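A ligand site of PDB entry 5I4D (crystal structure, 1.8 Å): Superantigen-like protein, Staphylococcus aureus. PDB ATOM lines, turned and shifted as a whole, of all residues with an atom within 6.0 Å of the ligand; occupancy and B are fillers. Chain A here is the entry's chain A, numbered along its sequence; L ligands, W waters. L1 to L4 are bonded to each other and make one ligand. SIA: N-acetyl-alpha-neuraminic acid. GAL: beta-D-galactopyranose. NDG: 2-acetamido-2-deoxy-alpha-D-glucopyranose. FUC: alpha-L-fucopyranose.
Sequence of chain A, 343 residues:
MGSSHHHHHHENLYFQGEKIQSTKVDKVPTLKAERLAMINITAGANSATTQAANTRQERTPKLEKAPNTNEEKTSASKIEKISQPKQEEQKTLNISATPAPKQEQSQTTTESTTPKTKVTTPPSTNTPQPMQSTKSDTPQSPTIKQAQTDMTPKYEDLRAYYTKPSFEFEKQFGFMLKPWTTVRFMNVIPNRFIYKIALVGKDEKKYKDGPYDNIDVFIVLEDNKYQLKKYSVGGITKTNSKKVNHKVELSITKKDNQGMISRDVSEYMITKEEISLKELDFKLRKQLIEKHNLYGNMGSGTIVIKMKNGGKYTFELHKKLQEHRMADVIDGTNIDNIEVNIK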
ATOM      1  N   LYS A 202     -20.144  -8.333 -19.749  1.00  0.00           N
ATOM      2  CA  LYS A 202     -20.619  -6.965 -20.108  1.00  0.00           C
ATOM      3  C   LYS A 202     -22.109  -6.748 -19.939  1.00  0.00           C
ATOM      4  O   LYS A 202     -22.577  -5.592 -19.874  1.00  0.00           O
ATOM      5  CB  LYS A 202     -20.231  -6.617 -21.555  1.00  0.00           C
ATOM      6  CG  LYS A 202     -18.727  -6.446 -21.790  1.00  0.00           C
ATOM      7  CD  LYS A 202     -18.409  -6.277 -23.265  1.00  0.00           C
ATOM      8  CE  LYS A 202     -16.904  -6.167 -23.510  1.00  0.00           C
ATOM      9  NZ  LYS A 202     -16.174  -7.454 -23.335  1.00  0.00           N
ATOM     10  N   LEU A 277     -20.999 -14.116 -29.347  1.00  0.00           N
ATOM     11  CA  LEU A 277     -19.948 -15.118 -29.436  1.00  0.00           C
ATOM     12  C   LEU A 277     -20.522 -16.461 -29.010  1.00  0.00           C
ATOM     13  O   LEU A 277     -20.106 -17.499 -29.521  1.00  0.00           O
ATOM     14  CB  LEU A 277     -18.728 -14.750 -28.623  1.00  0.00           C
ATOM     15  CG  LEU A 277     -17.993 -13.489 -29.040  1.00  0.00           C
ATOM     16  CD1 LEU A 277     -16.738 -13.354 -28.180  1.00  0.00           C
ATOM     17  CD2 LEU A 277     -17.613 -13.423 -30.505  1.00  0.00           C
ATOM     18  N   GLY A 311      -9.995  -7.089 -36.673  1.00  0.00           N
ATOM     19  CA  GLY A 311     -10.251  -7.751 -35.411  1.00  0.00           C
ATOM     20  C   GLY A 311     -10.396  -9.257 -35.551  1.00  0.00           C
ATOM     21  O   GLY A 311     -10.579  -9.800 -36.662  1.00  0.00           O
ATOM     22  N   LYS A 312     -10.279  -9.964 -34.424  1.00  0.00           N
ATOM     23  CA  LYS A 312     -10.502 -11.400 -34.402  1.00  0.00           C
ATOM     24  C   LYS A 312     -11.041 -11.848 -33.051  1.00  0.00           C
ATOM     25  O   LYS A 312     -10.834 -11.183 -32.040  1.00  0.00           O
ATOM     26  CB  LYS A 312      -9.225 -12.190 -34.740  1.00  0.00           C
ATOM     27  CG  LYS A 312      -8.196 -12.174 -33.643  1.00  0.00           C
ATOM     28  CD  LYS A 312      -6.968 -12.995 -34.016  1.00  0.00           C
ATOM     29  CE  LYS A 312      -6.039 -13.035 -32.802  1.00  0.00           C
ATOM     30  NZ  LYS A 312      -4.746 -13.678 -33.097  1.00  0.00           N
ATOM     31  N   TYR A 313     -11.686 -13.008 -33.068  1.00  0.00           N
ATOM     32  CA  TYR A 313     -12.279 -13.634 -31.867  1.00  0.00           C
ATOM     33  C   TYR A 313     -11.921 -15.116 -31.928  1.00  0.00           C
ATOM     34  O   TYR A 313     -12.177 -15.773 -32.913  1.00  0.00           O
ATOM     35  CB  TYR A 313     -13.766 -13.435 -31.790  1.00  0.00           C
ATOM     36  CG  TYR A 313     -14.155 -11.984 -31.822  1.00  0.00           C
ATOM     37  CD1 TYR A 313     -14.195 -11.216 -30.668  1.00  0.00           C
ATOM     38  CD2 TYR A 313     -14.393 -11.342 -33.047  1.00  0.00           C
ATOM     39  CE1 TYR A 313     -14.491  -9.864 -30.722  1.00  0.00           C
ATOM     40  CE2 TYR A 313     -14.703  -9.997 -33.094  1.00  0.00           C
ATOM     41  CZ  TYR A 313     -14.743  -9.260 -31.929  1.00  0.00           C
ATOM     42  OH  TYR A 313     -15.041  -7.939 -31.962  1.00  0.00           O
ATOM     43  N   THR A 314     -11.275 -15.585 -30.875  1.00  0.00           N
ATOM     44  CA  THR A 314     -10.763 -16.969 -30.818  1.00  0.00           C
ATOM     45  C   THR A 314     -11.482 -17.838 -29.817  1.00  0.00           C
ATOM     46  O   THR A 314     -11.632 -17.438 -28.616  1.00  0.00           O
ATOM     47  CB  THR A 314      -9.266 -16.943 -30.436  1.00  0.00           C
ATOM     48  OG1 THR A 314      -8.578 -16.081 -31.341  1.00  0.00           O
ATOM     49  CG2 THR A 314      -8.655 -18.322 -30.453  1.00  0.00           C
ATOM     50  N   PHE A 315     -11.925 -19.040 -30.274  1.00  0.00           N
ATOM     51  CA  PHE A 315     -12.538 -20.006 -29.406  1.00  0.00           C
ATOM     52  C   PHE A 315     -11.586 -21.200 -29.302  1.00  0.00           C
ATOM     53  O   PHE A 315     -11.294 -21.839 -30.288  1.00  0.00           O
ATOM     54  CB  PHE A 315     -13.888 -20.492 -29.943  1.00  0.00           C
ATOM     55  CG  PHE A 315     -14.826 -19.380 -30.355  1.00  0.00           C
ATOM     56  CD1 PHE A 315     -14.895 -18.193 -29.626  1.00  0.00           C
ATOM     57  CD2 PHE A 315     -15.665 -19.535 -31.434  1.00  0.00           C
ATOM     58  CE1 PHE A 315     -15.768 -17.188 -29.974  1.00  0.00           C
ATOM     59  CE2 PHE A 315     -16.541 -18.508 -31.825  1.00  0.00           C
ATOM     60  CZ  PHE A 315     -16.584 -17.336 -31.087  1.00  0.00           C
ATOM     61  N   GLU A 316     -11.131 -21.495 -28.102  1.00  0.00           N
ATOM     62  CA  GLU A 316     -10.233 -22.624 -27.848  1.00  0.00           C
ATOM     63  C   GLU A 316     -11.076 -23.914 -27.724  1.00  0.00           C
ATOM     64  O   GLU A 316     -11.913 -24.013 -26.838  1.00  0.00           O
ATOM     65  CB  GLU A 316      -9.440 -22.386 -26.566  1.00  0.00           C
ATOM     66  CG  GLU A 316      -8.553 -21.168 -26.602  1.00  0.00           C
ATOM     67  CD  GLU A 316      -7.750 -21.014 -25.337  1.00  0.00           C
ATOM     68  OE1 GLU A 316      -8.224 -20.316 -24.449  1.00  0.00           O
ATOM     69  OE2 GLU A 316      -6.706 -21.677 -25.183  1.00  0.00           O
ATOM     70  N   HIS A 318     -10.433 -27.011 -26.694  1.00  0.00           N
ATOM     71  CA  HIS A 318     -10.213 -28.000 -25.636  1.00  0.00           C
ATOM     72  C   HIS A 318     -11.019 -27.722 -24.360  1.00  0.00           C
ATOM     73  O   HIS A 318     -10.958 -28.524 -23.427  1.00  0.00           O
ATOM     74  CB  HIS A 318      -8.709 -28.116 -25.301  1.00  0.00           C
ATOM     75  CG  HIS A 318      -8.155 -26.892 -24.634  1.00  0.00           C
ATOM     76  ND1 HIS A 318      -7.797 -25.762 -25.331  1.00  0.00           N
ATOM     77  CD2 HIS A 318      -7.926 -26.610 -23.326  1.00  0.00           C
ATOM     78  CE1 HIS A 318      -7.349 -24.851 -24.491  1.00  0.00           C
ATOM     79  NE2 HIS A 318      -7.428 -25.331 -23.272  1.00  0.00           N
ATOM     80  N   LYS A 319     -11.773 -26.622 -24.339  1.00  0.00           N
ATOM     81  CA  LYS A 319     -12.623 -26.300 -23.203  1.00  0.00           C
ATOM     82  C   LYS A 319     -13.830 -25.482 -23.660  1.00  0.00           C
ATOM     83  O   LYS A 319     -13.869 -24.972 -24.790  1.00  0.00           O
ATOM     84  CB  LYS A 319     -11.826 -25.535 -22.139  1.00  0.00           C
ATOM     85  CG  LYS A 319     -11.294 -24.193 -22.568  1.00  0.00           C
ATOM     86  CD  LYS A 319     -10.494 -23.574 -21.438  1.00  0.00           C
ATOM     87  CE  LYS A 319     -10.026 -22.194 -21.772  1.00  0.00           C
ATOM     88  NZ  LYS A 319      -9.242 -21.675 -20.623  1.00  0.00           N
ATOM     89  N   GLN A 322     -15.480 -19.515 -22.272  1.00  0.00           N
ATOM     90  CA  GLN A 322     -15.614 -18.879 -20.934  1.00  0.00           C
ATOM     91  C   GLN A 322     -16.997 -18.244 -20.803  1.00  0.00           C
ATOM     92  O   GLN A 322     -17.445 -17.583 -21.716  1.00  0.00           O
ATOM     93  CB  GLN A 322     -14.511 -17.845 -20.723  1.00  0.00           C
ATOM     94  CG  GLN A 322     -13.055 -18.352 -20.835  1.00  0.00           C
ATOM     95  CD  GLN A 322     -12.421 -18.165 -22.214  1.00  0.00           C
ATOM     96  OE1 GLN A 322     -13.051 -18.341 -23.259  1.00  0.00           O
ATOM     97  NE2 GLN A 322     -11.129 -17.851 -22.224  1.00  0.00           N
ATOM     98  N   HIS A 324     -18.284 -15.590 -19.312  1.00  0.00           N
ATOM     99  CA  HIS A 324     -18.442 -14.167 -19.524  1.00  0.00           C
ATOM    100  C   HIS A 324     -18.430 -13.766 -20.992  1.00  0.00           C
ATOM    101  O   HIS A 324     -19.079 -12.782 -21.387  1.00  0.00           O
ATOM    102  CB  HIS A 324     -17.437 -13.350 -18.722  1.00  0.00           C
ATOM    103  CG  HIS A 324     -16.028 -13.509 -19.179  1.00  0.00           C
ATOM    104  ND1 HIS A 324     -15.217 -14.546 -18.755  1.00  0.00           N
ATOM    105  CD2 HIS A 324     -15.282 -12.773 -20.043  1.00  0.00           C
ATOM    106  CE1 HIS A 324     -14.028 -14.435 -19.325  1.00  0.00           C
ATOM    107  NE2 HIS A 324     -14.042 -13.374 -20.103  1.00  0.00           N
ATOM    108  N   ARG A 325     -17.717 -14.533 -21.806  1.00  0.00           N
ATOM    109  CA  ARG A 325     -17.637 -14.269 -23.240  1.00  0.00           C
ATOM    110  C   ARG A 325     -18.911 -14.629 -23.976  1.00  0.00           C
ATOM    111  O   ARG A 325     -19.128 -14.179 -25.086  1.00  0.00           O
ATOM    112  CB  ARG A 325     -16.429 -14.996 -23.830  1.00  0.00           C
ATOM    113  CG  ARG A 325     -15.095 -14.476 -23.288  1.00  0.00           C
ATOM    114  CD  ARG A 325     -13.922 -15.226 -23.920  1.00  0.00           C
ATOM    115  NE  ARG A 325     -13.772 -14.914 -25.344  1.00  0.00           N
ATOM    116  CZ  ARG A 325     -13.260 -15.731 -26.260  1.00  0.00           C
ATOM    117  NH1 ARG A 325     -12.882 -17.006 -25.973  1.00  0.00           N
ATOM    118  NH2 ARG A 325     -13.170 -15.302 -27.516  1.00  0.00           N
ATOM    119  N   ASP A 328     -20.605 -11.520 -24.908  1.00  0.00           N
ATOM    120  CA  ASP A 328     -19.999 -10.619 -25.901  1.00  0.00           C
ATOM    121  C   ASP A 328     -20.754 -10.679 -27.228  1.00  0.00           C
ATOM    122  O   ASP A 328     -21.173 -11.753 -27.679  1.00  0.00           O
ATOM    123  CB  ASP A 328     -18.510 -10.936 -26.101  1.00  0.00           C
ATOM    124  CG  ASP A 328     -17.636 -10.497 -24.913  1.00  0.00           C
ATOM    125  OD1 ASP A 328     -17.951  -9.474 -24.255  1.00  0.00           O
ATOM    126  OD2 ASP A 328     -16.598 -11.173 -24.646  1.00  0.00           O
HETATM  127  C1  SIA L   1      -9.148 -13.307 -29.122  1.00  0.00           C
HETATM  128  C2  SIA L   1      -8.690 -12.209 -28.157  1.00  0.00           C
HETATM  129  C3  SIA L   1      -7.746 -11.193 -28.789  1.00  0.00           C
HETATM  130  C4  SIA L   1      -8.439 -10.270 -29.771  1.00  0.00           C
HETATM  131  C5  SIA L   1      -9.710  -9.653 -29.187  1.00  0.00           C
HETATM  132  C6  SIA L   1     -10.567 -10.757 -28.548  1.00  0.00           C
HETATM  133  C7  SIA L   1     -11.815 -10.282 -27.818  1.00  0.00           C
HETATM  134  C8  SIA L   1     -12.494 -11.415 -27.052  1.00  0.00           C
HETATM  135  C9  SIA L   1     -13.887 -11.056 -26.552  1.00  0.00           C
HETATM  136  C10 SIA L   1     -10.823  -7.701 -30.170  1.00  0.00           C
HETATM  137  C11 SIA L   1     -11.582  -7.195 -31.352  1.00  0.00           C
HETATM  138  N5  SIA L   1     -10.445  -8.993 -30.239  1.00  0.00           N
HETATM  139  O1A SIA L   1     -10.308 -13.795 -28.964  1.00  0.00           O
HETATM  140  O1B SIA L   1      -8.369 -13.708 -29.975  1.00  0.00           O
HETATM  141  O4  SIA L   1      -7.557  -9.220 -30.181  1.00  0.00           O
HETATM  142  O6  SIA L   1      -9.784 -11.493 -27.595  1.00  0.00           O
HETATM  143  O7  SIA L   1     -11.463  -9.244 -26.895  1.00  0.00           O
HETATM  144  O8  SIA L   1     -12.559 -12.604 -27.864  1.00  0.00           O
HETATM  145  O9  SIA L   1     -14.438 -12.171 -25.841  1.00  0.00           O
HETATM  146  O10 SIA L   1     -10.538  -6.988 -29.209  1.00  0.00           O
HETATM  147  C1  GAL L   2      -9.238 -14.215 -23.894  1.00  0.00           C
HETATM  148  C2  GAL L   2      -8.376 -13.365 -24.819  1.00  0.00           C
HETATM  149  C3  GAL L   2      -8.762 -13.674 -26.258  1.00  0.00           C
HETATM  150  C4  GAL L   2      -8.529 -15.176 -26.514  1.00  0.00           C
HETATM  151  C5  GAL L   2      -9.312 -16.014 -25.491  1.00  0.00           C
HETATM  152  C6  GAL L   2      -9.026 -17.498 -25.668  1.00  0.00           C
HETATM  153  O2  GAL L   2      -8.517 -11.965 -24.513  1.00  0.00           O
HETATM  154  O3  GAL L   2      -7.959 -12.857 -27.117  1.00  0.00           O
HETATM  155  O4  GAL L   2      -7.124 -15.445 -26.478  1.00  0.00           O
HETATM  156  O5  GAL L   2      -9.025 -15.600 -24.147  1.00  0.00           O
HETATM  157  O6  GAL L   2      -9.825 -18.295 -24.808  1.00  0.00           O
HETATM  158  C1  NDG L   3     -10.710 -13.271 -18.882  1.00  0.00           C
HETATM  159  C2  NDG L   3     -10.260 -14.688 -19.230  1.00  0.00           C
HETATM  160  C3  NDG L   3      -9.255 -14.734 -20.376  1.00  0.00           C
HETATM  161  C4  NDG L   3      -9.861 -14.012 -21.568  1.00  0.00           C
HETATM  162  C5  NDG L   3     -10.340 -12.622 -21.176  1.00  0.00           C
HETATM  163  C6  NDG L   3     -11.103 -11.914 -22.280  1.00  0.00           C
HETATM  164  C7  NDG L   3     -10.454 -16.290 -17.407  1.00  0.00           C
HETATM  165  C8  NDG L   3      -9.884 -16.725 -16.085  1.00  0.00           C
HETATM  166  O5  NDG L   3     -11.241 -12.687 -20.059  1.00  0.00           O
HETATM  167  O3  NDG L   3      -8.979 -16.098 -20.715  1.00  0.00           O
HETATM  168  O4  NDG L   3      -8.867 -13.898 -22.574  1.00  0.00           O
HETATM  169  O6  NDG L   3     -12.303 -12.634 -22.526  1.00  0.00           O
HETATM  170  O7  NDG L   3     -11.493 -16.757 -17.871  1.00  0.00           O
HETATM  171  N2  NDG L   3      -9.780 -15.325 -18.026  1.00  0.00           N
HETATM  172  O1  NDG L   3      -9.640 -12.424 -18.406  1.00  0.00           O
HETATM  173  C1  FUC L   4      -7.779 -16.664 -20.140  1.00  0.00           C
HETATM  174  C2  FUC L   4      -7.785 -18.159 -20.447  1.00  0.00           C
HETATM  175  C3  FUC L   4      -7.475 -18.447 -21.916  1.00  0.00           C
HETATM  176  C4  FUC L   4      -6.231 -17.688 -22.378  1.00  0.00           C
HETATM  177  C5  FUC L   4      -6.345 -16.203 -22.034  1.00  0.00           C
HETATM  178  C6  FUC L   4      -5.063 -15.466 -22.390  1.00  0.00           C
HETATM  179  O2  FUC L   4      -9.070 -18.722 -20.106  1.00  0.00           O
HETATM  180  O3  FUC L   4      -7.298 -19.880 -22.085  1.00  0.00           O
HETATM  181  O4  FUC L   4      -5.053 -18.242 -21.757  1.00  0.00           O
HETATM  182  O5  FUC L   4      -6.594 -16.026 -20.628  1.00  0.00           O
HETATM  183  O   HOH W   1     -12.560 -19.142 -17.323  1.00  0.00           O
HETATM  184  O   HOH W   2      -6.291 -17.471 -27.743  1.00  0.00           O
HETATM  185  O   HOH W   3     -14.309 -10.768 -22.954  1.00  0.00           O
HETATM  186  O   HOH W   4      -5.161 -21.212 -20.833  1.00  0.00           O
HETATM  187  O   HOH W   5      -5.729 -14.168 -29.507  1.00  0.00           O
HETATM  188  O   HOH W   6     -11.904 -19.708 -25.978  1.00  0.00           O
HETATM  189  O   HOH W   7     -12.924 -10.342 -18.902  1.00  0.00           O
HETATM  190  O   HOH W   8     -12.831  -6.884 -27.441  1.00  0.00           O
HETATM  191  O   HOH W   9      -8.325  -8.172 -32.704  1.00  0.00           O
HETATM  192  O   HOH W  10      -8.646 -19.590 -17.660  1.00  0.00           O
HETATM  193  O   HOH W  11      -3.975 -19.551 -23.798  1.00  0.00           O
HETATM  194  O   HOH W  12      -9.855  -9.689 -19.058  1.00  0.00           O
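The side-chain carboxylate of Glu 316 is in hydrogen-bond range of an oxygen (O3) of FUC L4 (2.6 Å). An oxygen (O9) of SIA L1 lies within hydrogen-bond range of the side-chain carboxylate (OD2) of Asp 328 (2.7 Å). N of Thr 314 lies within hydrogen-bond range of O1A of SIA L1 (2.8 Å). The side-chain hydroxyl (OG1) of Thr 314 is in hydrogen-bond range of an oxygen (O1B) of SIA L1 (2.7 Å). The guanidinium group (NH2) of Arg 325 is in salt-bridge range of an oxygen (O1A) of SIA L1 (3.5 Å). A nitrogen (N5) of SIA L1 sits at hydrogen-bond distance from the backbone carbonyl oxygen of Lys 312, 2.9 Å away. NE2 of His 324 lies within hydrogen-bond range of O5 of NDG L3, 2.9 Å away. The side-chain amide nitrogen of Gln 322 sits at hydrogen-bond distance from an oxygen (O6) of GAL L2 (2.9 Å). NZ of Lys 319 sits at hydrogen-bond distance from O2 of FUC L4, 3.0 Å away.
The backbone carbonyl oxygen (O) of Asp 328 sits at hydrogen-bond distance from the backbone NH (N) of Leu 277 (2.9 Å). The side-chain carboxylate (OD1) of Asp 328 is in salt-bridge range of the side-chain amino group (NZ) of Lys 202 (2.8 Å). NH2 of Arg 325 is in hydrogen-bond range of O of Thr 314, at 2.9 Å. The side-chain amide oxygen of Gln 322 is in hydrogen-bond range of the guanidinium group of Arg 325.
Leu 277 touches the ligand. CA of Tyr 313 touches O1A of SIA L1, 3.5 Å away. Hydrophobic or aromatic side chains within 4 Å of the ligand: Leu 277, Tyr 313 and His 324. Within 4 Å of the ligand: Leu 277, Lys 312, Tyr 313, Thr 314, Glu 316, Lys 319, Gln 322, His 324, Arg 325 and Asp 328.
Water W6 lies within hydrogen-bond range of an oxygen (O6) of GAL L2 (2.8 Å), the guanidinium group (NH1) of Arg 325 (2.9 Å), the backbone NH (N) of Glu 316 (2.9 Å), the side-chain amide oxygen (OE1) of Gln 322 (3.3 Å) and the backbone carbonyl oxygen (O) of Thr 314 (3.5 Å). Water W3 lies within hydrogen-bond range of an oxygen (O6) of NDG L3 and the side-chain carboxylate of Asp 328. Water W9 bridges O4 of SIA L1 (2.8 Å) and N of Lys 312 (3.2 Å). Water W7 bridges an oxygen (O5) of NDG L3 (3.1 Å) and a ring nitrogen (NE2) of His 324 (3.4 Å).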
